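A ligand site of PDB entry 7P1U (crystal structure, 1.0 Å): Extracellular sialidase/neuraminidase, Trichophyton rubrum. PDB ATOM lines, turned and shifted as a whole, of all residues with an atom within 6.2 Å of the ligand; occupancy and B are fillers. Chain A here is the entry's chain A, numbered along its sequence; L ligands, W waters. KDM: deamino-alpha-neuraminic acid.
An oxygen (O1A) of the ligand is in salt-bridge range of the guanidinium group (NH2) of Arg 40, at 3.0 Å. O1B of the ligand is in salt-bridge range of NH2 of Arg 302, 2.8 Å away. OH of Tyr 338 is in hydrogen-bond range of O6 of the ligand (2.9 Å). The guanidinium group (NH2) of Arg 245 is in salt-bridge range of an oxygen (O1B) of the ligand, 2.9 Å away. An oxygen (O9) of the ligand sits at hydrogen-bond distance from the indole nitrogen (NE1) of Trp 182. NH2 of Arg 59 lies within hydrogen-bond range of O4 of the ligand, 2.9 Å away. An oxygen (O2) of the ligand sits at hydrogen-bond distance from the side-chain carboxylate (OD2) of Asp 65 (2.6 Å). The side-chain amide oxygen (OE1) of Gln 128 sits at hydrogen-bond distance from an oxygen (O7) of the ligand, 2.8 Å away.
The indole nitrogen (NE1) of Trp 182 sits close to the side-chain amide nitrogen (NE2) of Gln 128 (3.5 Å). The backbone NH (N) of Ile 41 is in hydrogen-bond range of the side-chain carboxylate (OE2) of Glu 354, 2.8 Å away. The backbone carbonyl oxygen (O) of Arg 40 lies within hydrogen-bond range of the backbone NH (N) of Glu 57 (2.8 Å). The guanidinium group (NH2) of Arg 245 is in hydrogen-bond range of the backbone carbonyl oxygen (O) of Ala 275, at 3.2 Å. N of Tyr 338 sits at hydrogen-bond distance from OE1 of Glu 354, at 2.8 Å. The side-chain hydroxyl (OH) of Tyr 338 is in hydrogen-bond range of the guanidinium group (NH1) of Arg 245 (2.8 Å). The guanidinium group of Arg 40 is in salt-bridge range of the side-chain carboxylate of Glu 354 (2.9 Å). The side-chain carboxylate (OE1) of Glu 229 lies within salt-bridge range of the guanidinium group (NH1) of Arg 245, at 2.8 Å.
Merely in contact with the ligand: Ile 41 (3.8 Å) and Glu 229 (3.4 Å). Hydrophobic or aromatic side chains within 4 Å of the ligand: Ile 41, Trp 182 and Tyr 338. Ten residues have an atom within 4 Å of the ligand: Arg 40, Ile 41, Arg 59, Asp 65, Gln 128, Trp 182, Glu 229, Arg 245, Arg 302 and Tyr 338. The nearest printed residue that does not touch the ligand is Ser 228 (4.2 Å).
Water W5 lies within hydrogen-bond range of an oxygen (O2) of the ligand and the side-chain carboxylate of Asp 65. Water W2 bridges O1A of the ligand and NH1 of Arg 302. Water W7 bridges an oxygen (O5) of the ligand (2.8 Å) and the guanidinium group of Arg 151 (3.4 Å). Water W6 lies within hydrogen-bond range of OG of Ser 228, O8 of the ligand and NE1 of Trp 182. Water W3 lies within hydrogen-bond range of OE2 of Glu 229, O5 of the ligand and ND2 of Asn 105. Water W1 bridges NH2 of Arg 302 (3.3 Å) and O1B of the ligand (3.3 Å).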
ATOM      1  N   ARG A  40      -7.378  28.564 -29.998  1.00  0.00           N
ATOM      2  CA  ARG A  40      -6.170  28.527 -30.783  1.00  0.00           C
ATOM      3  C   ARG A  40      -5.735  27.081 -30.916  1.00  0.00           C
ATOM      4  O   ARG A  40      -6.217  26.194 -30.206  1.00  0.00           O
ATOM      5  CB  ARG A  40      -5.052  29.369 -30.151  1.00  0.00           C
ATOM      6  CG  ARG A  40      -5.239  30.872 -30.304  1.00  0.00           C
ATOM      7  CD  ARG A  40      -3.905  31.619 -30.184  1.00  0.00           C
ATOM      8  NE  ARG A  40      -3.073  31.188 -31.292  1.00  0.00           N
ATOM      9  CZ  ARG A  40      -1.762  31.115 -31.278  1.00  0.00           C
ATOM     10  NH1 ARG A  40      -1.070  31.558 -30.260  1.00  0.00           N
ATOM     11  NH2 ARG A  40      -1.142  30.514 -32.266  1.00  0.00           N
ATOM     12  N   ILE A  41      -4.754  26.858 -31.781  1.00  0.00           N
ATOM     13  CA  ILE A  41      -3.987  25.618 -31.805  1.00  0.00           C
ATOM     14  C   ILE A  41      -4.853  24.435 -32.239  1.00  0.00           C
ATOM     15  O   ILE A  41      -5.083  23.483 -31.533  1.00  0.00           O
ATOM     16  CB  ILE A  41      -3.282  25.315 -30.478  1.00  0.00           C
ATOM     17  CG1 ILE A  41      -2.735  26.581 -29.784  1.00  0.00           C
ATOM     18  CG2 ILE A  41      -2.157  24.320 -30.741  1.00  0.00           C
ATOM     19  CD1 ILE A  41      -1.781  27.436 -30.579  1.00  0.00           C
ATOM     20  N   GLU A  57      -7.165  24.398 -28.333  1.00  0.00           N
ATOM     21  CA  GLU A  57      -7.016  24.972 -27.021  1.00  0.00           C
ATOM     22  C   GLU A  57      -8.126  25.988 -26.802  1.00  0.00           C
ATOM     23  O   GLU A  57      -8.264  26.955 -27.550  1.00  0.00           O
ATOM     24  CB  GLU A  57      -5.672  25.653 -26.887  1.00  0.00           C
ATOM     25  CG  GLU A  57      -4.545  24.666 -26.768  1.00  0.00           C
ATOM     26  CD  GLU A  57      -3.200  25.323 -26.662  1.00  0.00           C
ATOM     27  OE1 GLU A  57      -3.121  26.499 -26.227  1.00  0.00           O
ATOM     28  OE2 GLU A  57      -2.182  24.643 -27.011  1.00  0.00           O
ATOM     29  N   ARG A  59      -8.755  28.802 -24.576  1.00  0.00           N
ATOM     30  CA  ARG A  59      -7.948  29.695 -23.763  1.00  0.00           C
ATOM     31  C   ARG A  59      -8.940  30.577 -23.019  1.00  0.00           C
ATOM     32  O   ARG A  59      -9.634  31.411 -23.593  1.00  0.00           O
ATOM     33  CB  ARG A  59      -6.964  30.467 -24.644  1.00  0.00           C
ATOM     34  CG  ARG A  59      -6.012  29.527 -25.360  1.00  0.00           C
ATOM     35  CD  ARG A  59      -4.886  30.250 -26.047  1.00  0.00           C
ATOM     36  NE  ARG A  59      -3.877  29.316 -26.517  1.00  0.00           N
ATOM     37  CZ  ARG A  59      -2.668  29.658 -26.930  1.00  0.00           C
ATOM     38  NH1 ARG A  59      -2.311  30.923 -27.066  1.00  0.00           N
ATOM     39  NH2 ARG A  59      -1.767  28.719 -27.189  1.00  0.00           N
ATOM     40  N   ASP A  65      -0.595  31.916 -24.259  1.00  0.00           N
ATOM     41  CA  ASP A  65      -0.264  30.498 -24.356  1.00  0.00           C
ATOM     42  C   ASP A  65      -0.236  29.799 -23.026  1.00  0.00           C
ATOM     43  O   ASP A  65      -0.139  28.572 -22.979  1.00  0.00           O
ATOM     44  CB  ASP A  65       1.140  30.266 -24.950  1.00  0.00           C
ATOM     45  CG  ASP A  65       1.396  30.930 -26.300  1.00  0.00           C
ATOM     46  OD1 ASP A  65       0.444  31.317 -27.020  1.00  0.00           O
ATOM     47  OD2 ASP A  65       2.598  31.020 -26.602  1.00  0.00           O
ATOM     48  N   ASN A 105      -1.599  21.943 -27.179  1.00  0.00           N
ATOM     49  CA  ASN A 105      -0.828  21.296 -28.225  1.00  0.00           C
ATOM     50  C   ASN A 105      -1.440  19.997 -28.731  1.00  0.00           C
ATOM     51  O   ASN A 105      -0.755  18.996 -28.868  1.00  0.00           O
ATOM     52  CB  ASN A 105       0.630  21.042 -27.837  1.00  0.00           C
ATOM     53  CG  ASN A 105       1.476  22.293 -27.829  1.00  0.00           C
ATOM     54  OD1 ASN A 105       1.302  23.163 -26.978  1.00  0.00           O
ATOM     55  ND2 ASN A 105       2.406  22.397 -28.785  1.00  0.00           N
ATOM     56  N   GLN A 128       6.259  30.152 -20.624  1.00  0.00           N
ATOM     57  CA  GLN A 128       7.491  29.994 -21.372  1.00  0.00           C
ATOM     58  C   GLN A 128       8.524  31.022 -20.969  1.00  0.00           C
ATOM     59  O   GLN A 128       9.689  30.687 -20.782  1.00  0.00           O
ATOM     60  CB  GLN A 128       7.180  30.083 -22.863  1.00  0.00           C
ATOM     61  CG  GLN A 128       8.399  29.781 -23.710  1.00  0.00           C
ATOM     62  CD  GLN A 128       8.029  29.473 -25.126  1.00  0.00           C
ATOM     63  OE1 GLN A 128       6.959  29.851 -25.605  1.00  0.00           O
ATOM     64  NE2 GLN A 128       8.943  28.854 -25.843  1.00  0.00           N
ATOM     65  N   ARG A 151       7.607  21.628 -19.072  1.00  0.00           N
ATOM     66  CA  ARG A 151       6.495  21.199 -19.897  1.00  0.00           C
ATOM     67  C   ARG A 151       6.399  19.700 -19.924  1.00  0.00           C
ATOM     68  O   ARG A 151       7.395  18.999 -20.139  1.00  0.00           O
ATOM     69  CB  ARG A 151       6.656  21.751 -21.301  1.00  0.00           C
ATOM     70  CG  ARG A 151       6.382  23.262 -21.346  1.00  0.00           C
ATOM     71  CD  ARG A 151       4.936  23.572 -21.670  1.00  0.00           C
ATOM     72  NE  ARG A 151       4.741  23.405 -23.100  1.00  0.00           N
ATOM     73  CZ  ARG A 151       3.592  23.604 -23.720  1.00  0.00           C
ATOM     74  NH1 ARG A 151       2.505  23.916 -23.056  1.00  0.00           N
ATOM     75  NH2 ARG A 151       3.550  23.430 -25.021  1.00  0.00           N
ATOM     76  N   TRP A 182      11.235  23.767 -21.634  1.00  0.00           N
ATOM     77  CA  TRP A 182      10.157  23.918 -22.588  1.00  0.00           C
ATOM     78  C   TRP A 182      10.024  22.676 -23.427  1.00  0.00           C
ATOM     79  O   TRP A 182      10.992  21.953 -23.637  1.00  0.00           O
ATOM     80  CB  TRP A 182      10.371  25.155 -23.455  1.00  0.00           C
ATOM     81  CG  TRP A 182       9.234  25.429 -24.343  1.00  0.00           C
ATOM     82  CD1 TRP A 182       9.158  25.197 -25.697  1.00  0.00           C
ATOM     83  CD2 TRP A 182       7.957  25.937 -23.950  1.00  0.00           C
ATOM     84  NE1 TRP A 182       7.928  25.537 -26.151  1.00  0.00           N
ATOM     85  CE2 TRP A 182       7.161  25.981 -25.109  1.00  0.00           C
ATOM     86  CE3 TRP A 182       7.417  26.342 -22.742  1.00  0.00           C
ATOM     87  CZ2 TRP A 182       5.838  26.412 -25.089  1.00  0.00           C
ATOM     88  CZ3 TRP A 182       6.108  26.779 -22.724  1.00  0.00           C
ATOM     89  CH2 TRP A 182       5.339  26.813 -23.894  1.00  0.00           C
ATOM     90  N   ASP A 183       8.822  22.429 -23.917  1.00  0.00           N
ATOM     91  CA  ASP A 183       8.568  21.339 -24.819  1.00  0.00           C
ATOM     92  C   ASP A 183       7.310  21.644 -25.589  1.00  0.00           C
ATOM     93  O   ASP A 183       6.491  22.496 -25.189  1.00  0.00           O
ATOM     94  CB  ASP A 183       8.383  20.023 -24.098  1.00  0.00           C
ATOM     95  CG  ASP A 183       8.415  18.812 -25.023  1.00  0.00           C
ATOM     96  OD1 ASP A 183       9.162  18.856 -26.031  1.00  0.00           O
ATOM     97  OD2 ASP A 183       7.701  17.835 -24.710  1.00  0.00           O
ATOM     98  N   ALA A 184       7.131  20.922 -26.686  1.00  0.00           N
ATOM     99  CA  ALA A 184       5.916  20.956 -27.479  1.00  0.00           C
ATOM    100  C   ALA A 184       5.759  19.624 -28.148  1.00  0.00           C
ATOM    101  O   ALA A 184       6.749  19.022 -28.551  1.00  0.00           O
ATOM    102  CB  ALA A 184       5.983  22.044 -28.534  1.00  0.00           C
ATOM    103  N   GLN A 203       8.982  18.506 -30.275  1.00  0.00           N
ATOM    104  CA  GLN A 203      10.159  19.337 -30.271  1.00  0.00           C
ATOM    105  C   GLN A 203      11.409  18.503 -30.223  1.00  0.00           C
ATOM    106  O   GLN A 203      11.608  17.658 -29.328  1.00  0.00           O
ATOM    107  CB  GLN A 203      10.131  20.270 -29.053  1.00  0.00           C
ATOM    108  CG  GLN A 203      11.455  21.007 -28.862  1.00  0.00           C
ATOM    109  CD  GLN A 203      11.370  22.109 -27.834  1.00  0.00           C
ATOM    110  OE1 GLN A 203      10.446  22.900 -27.843  1.00  0.00           O
ATOM    111  NE2 GLN A 203      12.335  22.160 -26.937  1.00  0.00           N
ATOM    112  N   SER A 228      10.728  23.104 -32.811  1.00  0.00           N
ATOM    113  CA  SER A 228       9.829  22.911 -31.689  1.00  0.00           C
ATOM    114  C   SER A 228       8.490  22.417 -32.150  1.00  0.00           C
ATOM    115  O   SER A 228       7.969  21.466 -31.562  1.00  0.00           O
ATOM    116  CB  SER A 228       9.732  24.189 -30.845  1.00  0.00           C
ATOM    117  OG  SER A 228       8.881  23.956 -29.744  1.00  0.00           O
ATOM    118  N   GLU A 229       7.935  23.074 -33.153  1.00  0.00           N
ATOM    119  CA  GLU A 229       6.651  22.721 -33.710  1.00  0.00           C
ATOM    120  C   GLU A 229       6.852  22.096 -35.075  1.00  0.00           C
ATOM    121  O   GLU A 229       7.102  22.787 -36.084  1.00  0.00           O
ATOM    122  CB  GLU A 229       5.735  23.921 -33.842  1.00  0.00           C
ATOM    123  CG  GLU A 229       5.305  24.465 -32.472  1.00  0.00           C
ATOM    124  CD  GLU A 229       4.386  25.656 -32.603  1.00  0.00           C
ATOM    125  OE1 GLU A 229       4.354  26.276 -33.685  1.00  0.00           O
ATOM    126  OE2 GLU A 229       3.706  25.961 -31.598  1.00  0.00           O
ATOM    127  N   ARG A 245       8.400  24.405 -38.223  1.00  0.00           N
ATOM    128  CA  ARG A 245       8.425  25.821 -37.992  1.00  0.00           C
ATOM    129  C   ARG A 245       9.862  26.224 -37.683  1.00  0.00           C
ATOM    130  O   ARG A 245      10.505  25.628 -36.822  1.00  0.00           O
ATOM    131  CB  ARG A 245       7.547  26.139 -36.791  1.00  0.00           C
ATOM    132  CG  ARG A 245       7.658  27.546 -36.275  1.00  0.00           C
ATOM    133  CD  ARG A 245       6.771  27.748 -35.095  1.00  0.00           C
ATOM    134  NE  ARG A 245       6.948  29.057 -34.486  1.00  0.00           N
ATOM    135  CZ  ARG A 245       6.077  29.599 -33.655  1.00  0.00           C
ATOM    136  NH1 ARG A 245       4.903  29.048 -33.410  1.00  0.00           N
ATOM    137  NH2 ARG A 245       6.373  30.769 -33.075  1.00  0.00           N
ATOM    138  N   ALA A 275       7.696  32.076 -39.024  1.00  0.00           N
ATOM    139  CA  ALA A 275       7.868  31.432 -37.720  1.00  0.00           C
ATOM    140  C   ALA A 275       6.511  31.183 -37.102  1.00  0.00           C
ATOM    141  O   ALA A 275       6.119  31.802 -36.113  1.00  0.00           O
ATOM    142  CB  ALA A 275       8.847  32.162 -36.787  1.00  0.00           C
ATOM    143  N   CYS A 276       5.779  30.294 -37.740  1.00  0.00           N
ATOM    144  CA  CYS A 276       4.471  29.881 -37.314  1.00  0.00           C
ATOM    145  C   CYS A 276       4.308  28.410 -37.600  1.00  0.00           C
ATOM    146  O   CYS A 276       4.999  27.872 -38.477  1.00  0.00           O
ATOM    147  CB  CYS A 276       3.429  30.712 -38.042  1.00  0.00           C
ATOM    148  SG  CYS A 276       1.726  30.494 -37.549  1.00  0.00           S
ATOM    149  N   ARG A 302       1.343  36.234 -40.560  1.00  0.00           N
ATOM    150  CA  ARG A 302       0.561  35.008 -40.515  1.00  0.00           C
ATOM    151  C   ARG A 302      -0.724  35.062 -41.344  1.00  0.00           C
ATOM    152  O   ARG A 302      -1.459  34.076 -41.391  1.00  0.00           O
ATOM    153  CB  ARG A 302       0.194  34.680 -39.062  1.00  0.00           C
ATOM    154  CG  ARG A 302       1.411  34.309 -38.233  1.00  0.00           C
ATOM    155  CD  ARG A 302       1.129  33.927 -36.813  1.00  0.00           C
ATOM    156  NE  ARG A 302       2.363  33.510 -36.173  1.00  0.00           N
ATOM    157  CZ  ARG A 302       2.427  32.877 -35.002  1.00  0.00           C
ATOM    158  NH1 ARG A 302       1.363  32.603 -34.284  1.00  0.00           N
ATOM    159  NH2 ARG A 302       3.616  32.597 -34.520  1.00  0.00           N
ATOM    160  N   TYR A 338      -1.996  29.169 -37.166  1.00  0.00           N
ATOM    161  CA  TYR A 338      -1.838  27.726 -37.156  1.00  0.00           C
ATOM    162  C   TYR A 338      -2.971  27.082 -37.964  1.00  0.00           C
ATOM    163  O   TYR A 338      -4.085  27.618 -38.099  1.00  0.00           O
ATOM    164  CB  TYR A 338      -1.911  27.210 -35.722  1.00  0.00           C
ATOM    165  CG  TYR A 338      -0.725  27.480 -34.860  1.00  0.00           C
ATOM    166  CD1 TYR A 338       0.036  28.647 -34.920  1.00  0.00           C
ATOM    167  CD2 TYR A 338      -0.363  26.544 -33.900  1.00  0.00           C
ATOM    168  CE1 TYR A 338       1.113  28.847 -34.074  1.00  0.00           C
ATOM    169  CE2 TYR A 338       0.714  26.744 -33.044  1.00  0.00           C
ATOM    170  CZ  TYR A 338       1.441  27.910 -33.131  1.00  0.00           C
ATOM    171  OH  TYR A 338       2.462  28.162 -32.265  1.00  0.00           O
ATOM    172  N   GLU A 354      -6.587  29.172 -37.873  1.00  0.00           N
ATOM    173  CA  GLU A 354      -6.750  30.241 -36.907  1.00  0.00           C
ATOM    174  C   GLU A 354      -7.131  31.566 -37.564  1.00  0.00           C
ATOM    175  O   GLU A 354      -6.743  31.846 -38.702  1.00  0.00           O
ATOM    176  CB  GLU A 354      -5.457  30.465 -36.140  1.00  0.00           C
ATOM    177  CG  GLU A 354      -5.132  29.337 -35.203  1.00  0.00           C
ATOM    178  CD  GLU A 354      -3.926  29.632 -34.344  1.00  0.00           C
ATOM    179  OE1 GLU A 354      -2.982  30.321 -34.834  1.00  0.00           O
ATOM    180  OE2 GLU A 354      -3.880  29.164 -33.185  1.00  0.00           O
ATOM    181  N   ARG A 368      -9.410  35.225 -30.476  1.00  0.00           N
ATOM    182  CA  ARG A 368      -9.011  34.300 -31.532  1.00  0.00           C
ATOM    183  C   ARG A 368     -10.081  33.261 -31.750  1.00  0.00           C
ATOM    184  O   ARG A 368     -10.610  32.716 -30.761  1.00  0.00           O
ATOM    185  CB  ARG A 368      -7.696  33.611 -31.199  1.00  0.00           C
ATOM    186  CG  ARG A 368      -6.615  34.517 -30.680  1.00  0.00           C
ATOM    187  CD  ARG A 368      -6.217  35.572 -31.688  1.00  0.00           C
ATOM    188  NE  ARG A 368      -5.052  36.335 -31.255  1.00  0.00           N
ATOM    189  CZ  ARG A 368      -3.796  35.907 -31.360  1.00  0.00           C
ATOM    190  NH1 ARG A 368      -3.514  34.710 -31.833  1.00  0.00           N
ATOM    191  NH2 ARG A 368      -2.805  36.692 -30.976  1.00  0.00           N
HETATM  192  C2  KDM L   1       2.981  30.378 -30.083  1.00  0.00           C
HETATM  193  C1  KDM L   1       2.786  31.195 -31.328  1.00  0.00           C
HETATM  194  C3  KDM L   1       1.702  29.629 -29.734  1.00  0.00           C
HETATM  195  C4  KDM L   1       1.963  28.338 -28.940  1.00  0.00           C
HETATM  196  C5  KDM L   1       3.317  28.289 -28.247  1.00  0.00           C
HETATM  197  C6  KDM L   1       4.401  28.432 -29.349  1.00  0.00           C
HETATM  198  C7  KDM L   1       5.810  28.695 -28.846  1.00  0.00           C
HETATM  199  C8  KDM L   1       6.846  28.790 -29.940  1.00  0.00           C
HETATM  200  C9  KDM L   1       8.231  29.067 -29.386  1.00  0.00           C
HETATM  201  O5  KDM L   1       3.479  27.057 -27.520  1.00  0.00           O
HETATM  202  O1A KDM L   1       1.641  31.406 -31.728  1.00  0.00           O
HETATM  203  O1B KDM L   1       3.803  31.586 -31.901  1.00  0.00           O
HETATM  204  O4  KDM L   1       0.927  28.143 -27.988  1.00  0.00           O
HETATM  205  O6  KDM L   1       4.100  29.509 -30.284  1.00  0.00           O
HETATM  206  O7  KDM L   1       5.839  29.928 -28.119  1.00  0.00           O
HETATM  207  O8  KDM L   1       6.877  27.579 -30.664  1.00  0.00           O
HETATM  208  O9  KDM L   1       8.632  28.014 -28.500  1.00  0.00           O
HETATM  209  O2  KDM L   1       3.363  31.275 -29.086  1.00  0.00           O
HETATM  210  O   HOH W   1       3.876  34.868 -32.151  1.00  0.00           O
HETATM  211  O   HOH W   2       1.507  34.020 -31.116  1.00  0.00           O
HETATM  212  O   HOH W   3       4.028  24.843 -29.152  1.00  0.00           O
HETATM  213  O   HOH W   4       5.787  32.233 -29.601  1.00  0.00           O
HETATM  214  O   HOH W   5       4.028  33.566 -28.058  1.00  0.00           O
HETATM  215  O   HOH W   6       6.759  25.414 -28.907  1.00  0.00           O
HETATM  216  O   HOH W   7       2.066  26.574 -25.169  1.00  0.00           O
HETATM  217  O   HOH W   8       0.237  25.615 -27.919  1.00  0.00           O
